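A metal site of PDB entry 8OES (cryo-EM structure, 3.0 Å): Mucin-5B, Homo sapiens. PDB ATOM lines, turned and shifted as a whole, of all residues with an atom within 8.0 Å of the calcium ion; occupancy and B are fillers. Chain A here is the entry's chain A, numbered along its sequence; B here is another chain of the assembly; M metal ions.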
ATOM      1  N   THR A 880      19.504 -35.586  24.816  1.00  0.00           N
ATOM      2  CA  THR A 880      19.153 -34.210  24.525  1.00  0.00           C
ATOM      3  C   THR A 880      19.941 -33.696  23.333  1.00  0.00           C
ATOM      4  O   THR A 880      20.697 -34.414  22.684  1.00  0.00           O
ATOM      5  CB  THR A 880      19.403 -33.331  25.740  1.00  0.00           C
ATOM      6  OG1 THR A 880      19.612 -31.983  25.284  1.00  0.00           O
ATOM      7  CG2 THR A 880      20.617 -33.785  26.475  1.00  0.00           C
ATOM      8  N   PHE A 881      19.718 -32.413  23.039  1.00  0.00           N
ATOM      9  CA  PHE A 881      20.320 -31.806  21.866  1.00  0.00           C
ATOM     10  C   PHE A 881      21.841 -31.781  21.969  1.00  0.00           C
ATOM     11  O   PHE A 881      22.536 -32.023  20.986  1.00  0.00           O
ATOM     12  CB  PHE A 881      19.785 -30.382  21.694  1.00  0.00           C
ATOM     13  CG  PHE A 881      18.435 -30.305  21.035  1.00  0.00           C
ATOM     14  CD1 PHE A 881      18.267 -30.637  19.712  1.00  0.00           C
ATOM     15  CD2 PHE A 881      17.342 -29.860  21.751  1.00  0.00           C
ATOM     16  CE1 PHE A 881      17.030 -30.543  19.123  1.00  0.00           C
ATOM     17  CE2 PHE A 881      16.105 -29.766  21.162  1.00  0.00           C
ATOM     18  CZ  PHE A 881      15.953 -30.108  19.851  1.00  0.00           C
ATOM     19  N   ASP A 882      22.361 -31.471  23.157  1.00  0.00           N
ATOM     20  CA  ASP A 882      23.789 -31.345  23.397  1.00  0.00           C
ATOM     21  C   ASP A 882      24.478 -32.696  23.567  1.00  0.00           C
ATOM     22  O   ASP A 882      25.631 -32.719  23.997  1.00  0.00           O
ATOM     23  CB  ASP A 882      24.052 -30.499  24.643  1.00  0.00           C
ATOM     24  CG  ASP A 882      23.549 -29.094  24.497  1.00  0.00           C
ATOM     25  OD1 ASP A 882      23.793 -28.476  23.451  1.00  0.00           O
ATOM     26  OD2 ASP A 882      22.882 -28.617  25.431  1.00  0.00           O
ATOM     27  N   ASP A 884      23.877 -35.158  25.693  1.00  0.00           N
ATOM     28  CA  ASP A 884      23.773 -35.830  26.984  1.00  0.00           C
ATOM     29  C   ASP A 884      22.719 -36.926  26.930  1.00  0.00           C
ATOM     30  O   ASP A 884      21.754 -36.851  26.173  1.00  0.00           O
ATOM     31  CB  ASP A 884      23.438 -34.827  28.085  1.00  0.00           C
ATOM     32  CG  ASP A 884      23.558 -35.417  29.458  1.00  0.00           C
ATOM     33  OD1 ASP A 884      23.976 -36.586  29.575  1.00  0.00           O
ATOM     34  OD2 ASP A 884      23.232 -34.723  30.439  1.00  0.00           O
ATOM     35  N   GLY A 995      20.605 -22.444  21.887  1.00  0.00           N
ATOM     36  CA  GLY A 995      20.714 -21.723  23.136  1.00  0.00           C
ATOM     37  C   GLY A 995      19.437 -21.114  23.651  1.00  0.00           C
ATOM     38  O   GLY A 995      19.425 -20.599  24.784  1.00  0.00           O
ATOM     39  N   CYS A1001      14.868 -31.655  26.447  1.00  0.00           N
ATOM     40  CA  CYS A1001      15.924 -31.781  25.446  1.00  0.00           C
ATOM     41  C   CYS A1001      17.035 -30.764  25.688  1.00  0.00           C
ATOM     42  O   CYS A1001      17.703 -30.341  24.737  1.00  0.00           O
ATOM     43  CB  CYS A1001      15.360 -31.618  24.038  1.00  0.00           C
ATOM     44  SG  CYS A1001      14.135 -32.853  23.557  1.00  0.00           S
ATOM     45  N   GLY A1002      17.243 -30.375  26.939  1.00  0.00           N
ATOM     46  CA  GLY A1002      18.297 -29.448  27.256  1.00  0.00           C
ATOM     47  C   GLY A1002      17.993 -28.078  26.684  1.00  0.00           C
ATOM     48  O   GLY A1002      16.886 -27.784  26.260  1.00  0.00           O
ATOM     49  N   ASN A1003      19.028 -27.244  26.690  1.00  0.00           N
ATOM     50  CA  ASN A1003      18.899 -25.893  26.153  1.00  0.00           C
ATOM     51  C   ASN A1003      19.682 -25.693  24.869  1.00  0.00           C
ATOM     52  O   ASN A1003      19.808 -24.562  24.416  1.00  0.00           O
ATOM     53  CB  ASN A1003      19.326 -24.874  27.209  1.00  0.00           C
ATOM     54  CG  ASN A1003      20.809 -24.874  27.453  1.00  0.00           C
ATOM     55  OD1 ASN A1003      21.456 -25.913  27.386  1.00  0.00           O
ATOM     56  ND2 ASN A1003      21.356 -23.714  27.760  1.00  0.00           N
ATOM     57  N   PHE A1004      20.191 -26.770  24.267  1.00  0.00           N
ATOM     58  CA  PHE A1004      20.836 -26.701  22.970  1.00  0.00           C
ATOM     59  C   PHE A1004      21.912 -25.621  22.942  1.00  0.00           C
ATOM     60  O   PHE A1004      21.829 -24.644  22.204  1.00  0.00           O
ATOM     61  CB  PHE A1004      19.792 -26.458  21.873  1.00  0.00           C
ATOM     62  CG  PHE A1004      20.294 -26.693  20.484  1.00  0.00           C
ATOM     63  CD1 PHE A1004      21.491 -27.312  20.255  1.00  0.00           C
ATOM     64  CD2 PHE A1004      19.528 -26.298  19.398  1.00  0.00           C
ATOM     65  CE1 PHE A1004      21.928 -27.529  18.963  1.00  0.00           C
ATOM     66  CE2 PHE A1004      19.973 -26.515  18.113  1.00  0.00           C
ATOM     67  CZ  PHE A1004      21.169 -27.127  17.899  1.00  0.00           C
ATOM     68  N   ASP A1005      22.922 -25.803  23.784  1.00  0.00           N
ATOM     69  CA  ASP A1005      23.986 -24.817  23.902  1.00  0.00           C
ATOM     70  C   ASP A1005      25.369 -25.392  23.623  1.00  0.00           C
ATOM     71  O   ASP A1005      26.370 -24.704  23.839  1.00  0.00           O
ATOM     72  CB  ASP A1005      23.964 -24.165  25.288  1.00  0.00           C
ATOM     73  CG  ASP A1005      24.136 -25.172  26.412  1.00  0.00           C
ATOM     74  OD1 ASP A1005      24.026 -26.384  26.140  1.00  0.00           O
ATOM     75  OD2 ASP A1005      24.381 -24.752  27.552  1.00  0.00           O
ATOM     76  N   ASP A1006      25.448 -26.642  23.155  1.00  0.00           N
ATOM     77  CA  ASP A1006      26.717 -27.354  23.011  1.00  0.00           C
ATOM     78  C   ASP A1006      27.493 -27.361  24.327  1.00  0.00           C
ATOM     79  O   ASP A1006      28.703 -27.178  24.361  1.00  0.00           O
ATOM     80  CB  ASP A1006      27.563 -26.749  21.886  1.00  0.00           C
ATOM     81  CG  ASP A1006      26.757 -26.433  20.656  1.00  0.00           C
ATOM     82  OD1 ASP A1006      25.786 -25.663  20.776  1.00  0.00           O
ATOM     83  OD2 ASP A1006      27.092 -26.959  19.576  1.00  0.00           O
ATOM     84  N   ASN A1007      26.760 -27.577  25.414  1.00  0.00           N
ATOM     85  CA  ASN A1007      27.355 -27.663  26.746  1.00  0.00           C
ATOM     86  C   ASN A1007      26.498 -28.659  27.513  1.00  0.00           C
ATOM     87  O   ASN A1007      25.485 -28.289  28.116  1.00  0.00           O
ATOM     88  CB  ASN A1007      27.407 -26.313  27.438  1.00  0.00           C
ATOM     89  CG  ASN A1007      27.992 -26.377  28.823  1.00  0.00           C
ATOM     90  OD1 ASN A1007      28.245 -27.454  29.357  1.00  0.00           O
ATOM     91  ND2 ASN A1007      28.213 -25.214  29.427  1.00  0.00           N
ATOM     92  N   ALA A1008      26.913 -29.921  27.488  1.00  0.00           N
ATOM     93  CA  ALA A1008      26.066 -31.009  27.971  1.00  0.00           C
ATOM     94  C   ALA A1008      26.118 -31.179  29.481  1.00  0.00           C
ATOM     95  O   ALA A1008      25.272 -31.888  30.028  1.00  0.00           O
ATOM     96  CB  ALA A1008      26.465 -32.317  27.299  1.00  0.00           C
ATOM     97  N   ILE A1009      27.079 -30.561  30.160  1.00  0.00           N
ATOM     98  CA  ILE A1009      27.175 -30.744  31.595  1.00  0.00           C
ATOM     99  C   ILE A1009      26.036 -30.041  32.311  1.00  0.00           C
ATOM    100  O   ILE A1009      25.481 -30.553  33.289  1.00  0.00           O
ATOM    101  CB  ILE A1009      28.548 -30.267  32.106  1.00  0.00           C
ATOM    102  CG1 ILE A1009      29.605 -30.409  31.003  1.00  0.00           C
ATOM    103  CG2 ILE A1009      28.954 -31.069  33.328  1.00  0.00           C
ATOM    104  CD1 ILE A1009      30.936 -29.805  31.368  1.00  0.00           C
ATOM    105  N   ASN A1010      25.647 -28.859  31.832  1.00  0.00           N
ATOM    106  CA  ASN A1010      24.634 -28.045  32.473  1.00  0.00           C
ATOM    107  C   ASN A1010      23.241 -28.250  31.892  1.00  0.00           C
ATOM    108  O   ASN A1010      22.326 -27.493  32.229  1.00  0.00           O
ATOM    109  CB  ASN A1010      25.014 -26.561  32.401  1.00  0.00           C
ATOM    110  CG  ASN A1010      24.437 -25.868  31.199  1.00  0.00           C
ATOM    111  OD1 ASN A1010      24.539 -26.361  30.073  1.00  0.00           O
ATOM    112  ND2 ASN A1010      23.800 -24.728  31.428  1.00  0.00           N
ATOM    113  N   ASP A1011      23.057 -29.250  31.030  1.00  0.00           N
ATOM    114  CA  ASP A1011      21.747 -29.485  30.449  1.00  0.00           C
ATOM    115  C   ASP A1011      20.728 -29.947  31.463  1.00  0.00           C
ATOM    116  O   ASP A1011      19.536 -29.986  31.147  1.00  0.00           O
ATOM    117  CB  ASP A1011      21.833 -30.500  29.319  1.00  0.00           C
ATOM    118  CG  ASP A1011      21.652 -29.883  27.980  1.00  0.00           C
ATOM    119  OD1 ASP A1011      21.781 -28.639  27.898  1.00  0.00           O
ATOM    120  OD2 ASP A1011      21.382 -30.603  27.001  1.00  0.00           O
ATOM    121  N   PHE A1012      21.149 -30.316  32.664  1.00  0.00           N
ATOM    122  CA  PHE A1012      20.197 -30.603  33.734  1.00  0.00           C
ATOM    123  C   PHE A1012      19.778 -29.309  34.413  1.00  0.00           C
ATOM    124  O   PHE A1012      19.869 -29.188  35.632  1.00  0.00           O
ATOM    125  CB  PHE A1012      20.816 -31.550  34.752  1.00  0.00           C
ATOM    126  CG  PHE A1012      20.724 -32.991  34.377  1.00  0.00           C
ATOM    127  CD1 PHE A1012      20.592 -33.369  33.061  1.00  0.00           C
ATOM    128  CD2 PHE A1012      20.755 -33.976  35.345  1.00  0.00           C
ATOM    129  CE1 PHE A1012      20.512 -34.690  32.717  1.00  0.00           C
ATOM    130  CE2 PHE A1012      20.659 -35.291  35.016  1.00  0.00           C
ATOM    131  CZ  PHE A1012      20.532 -35.658  33.694  1.00  0.00           C
ATOM    132  N   ALA A1013      19.311 -28.351  33.627  1.00  0.00           N
ATOM    133  CA  ALA A1013      18.876 -27.057  34.135  1.00  0.00           C
ATOM    134  C   ALA A1013      17.371 -27.068  34.318  1.00  0.00           C
ATOM    135  O   ALA A1013      16.618 -27.187  33.342  1.00  0.00           O
ATOM    136  CB  ALA A1013      19.298 -25.936  33.185  1.00  0.00           C
ATOM    137  N   VAL A1019      21.222 -25.813  37.970  1.00  0.00           N
ATOM    138  CA  VAL A1019      21.741 -27.053  37.374  1.00  0.00           C
ATOM    139  C   VAL A1019      21.972 -28.077  38.465  1.00  0.00           C
ATOM    140  O   VAL A1019      22.685 -27.831  39.438  1.00  0.00           O
ATOM    141  CB  VAL A1019      23.027 -26.777  36.591  1.00  0.00           C
ATOM    142  CG1 VAL A1019      23.780 -28.063  36.360  1.00  0.00           C
ATOM    143  CG2 VAL A1019      22.684 -26.124  35.262  1.00  0.00           C
ATOM    144  N   GLN B 542      33.982 -27.205  27.582  1.00  0.00           N
ATOM    145  CA  GLN B 542      32.592 -27.335  28.010  1.00  0.00           C
ATOM    146  C   GLN B 542      31.691 -27.725  26.845  1.00  0.00           C
ATOM    147  O   GLN B 542      30.747 -27.037  26.475  1.00  0.00           O
ATOM    148  CB  GLN B 542      32.117 -26.050  28.689  1.00  0.00           C
ATOM    149  CG  GLN B 542      33.108 -25.468  29.668  1.00  0.00           C
ATOM    150  CD  GLN B 542      33.705 -26.516  30.580  1.00  0.00           C
ATOM    151  OE1 GLN B 542      33.026 -27.440  31.015  1.00  0.00           O
ATOM    152  NE2 GLN B 542      34.972 -26.354  30.902  1.00  0.00           N
HETATM  153 CA    CA M   1      23.508 -27.052  28.138  1.00  0.00          CA
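The backbone NH (N) of Asp 1005 lies within hydrogen-bond range of the side-chain carboxylate (OD1) of Asp 882. OD1 of Asn 1007 lies close to N of Ile 1009, 3.4 Å away. The side-chain carboxylate (OD2) of Asp 882 lies close to the side-chain carboxylate (OD1) of Asp 1011. The side-chain hydroxyl (OG1) of Thr 880 sits at hydrogen-bond distance from the side-chain carboxylate (OD2) of Asp 1011, at 2.8 Å. The backbone carbonyl oxygen (O) of Asn 1003 sits close to the backbone NH (N) of Gly 995, 3.4 Å away. N of Phe 1004 sits at hydrogen-bond distance from OD2 of Asp 882 (3.5 Å). OD1 of Asp 882 sits at hydrogen-bond distance from N of Asp 1006 (2.5 Å).
Residues that only touch the calcium ion: Asp 882 (3.2 Å). Of the 20 residues printed, 6 come within 4 Å of the calcium ion. The nearest printed residue that does not touch the calcium ion is Ala 1008 (4.5 Å).
The calcium ion is bound by the side-chain carboxylate (OD1) of Asp 1005 (2.2 Å), the side-chain amide oxygen (OD1) of Asn 1010 (2.3 Å), the backbone carbonyl oxygen (O) of Asn 1007 (2.3 Å), the side-chain carboxylate (OD1) of Asp 1011 (2.4 Å), the side-chain amide oxygen (OD1) of Asn 1003 (2.5 Å) and the side-chain carboxylate (OD2) of Asp 1005 (2.5 Å).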
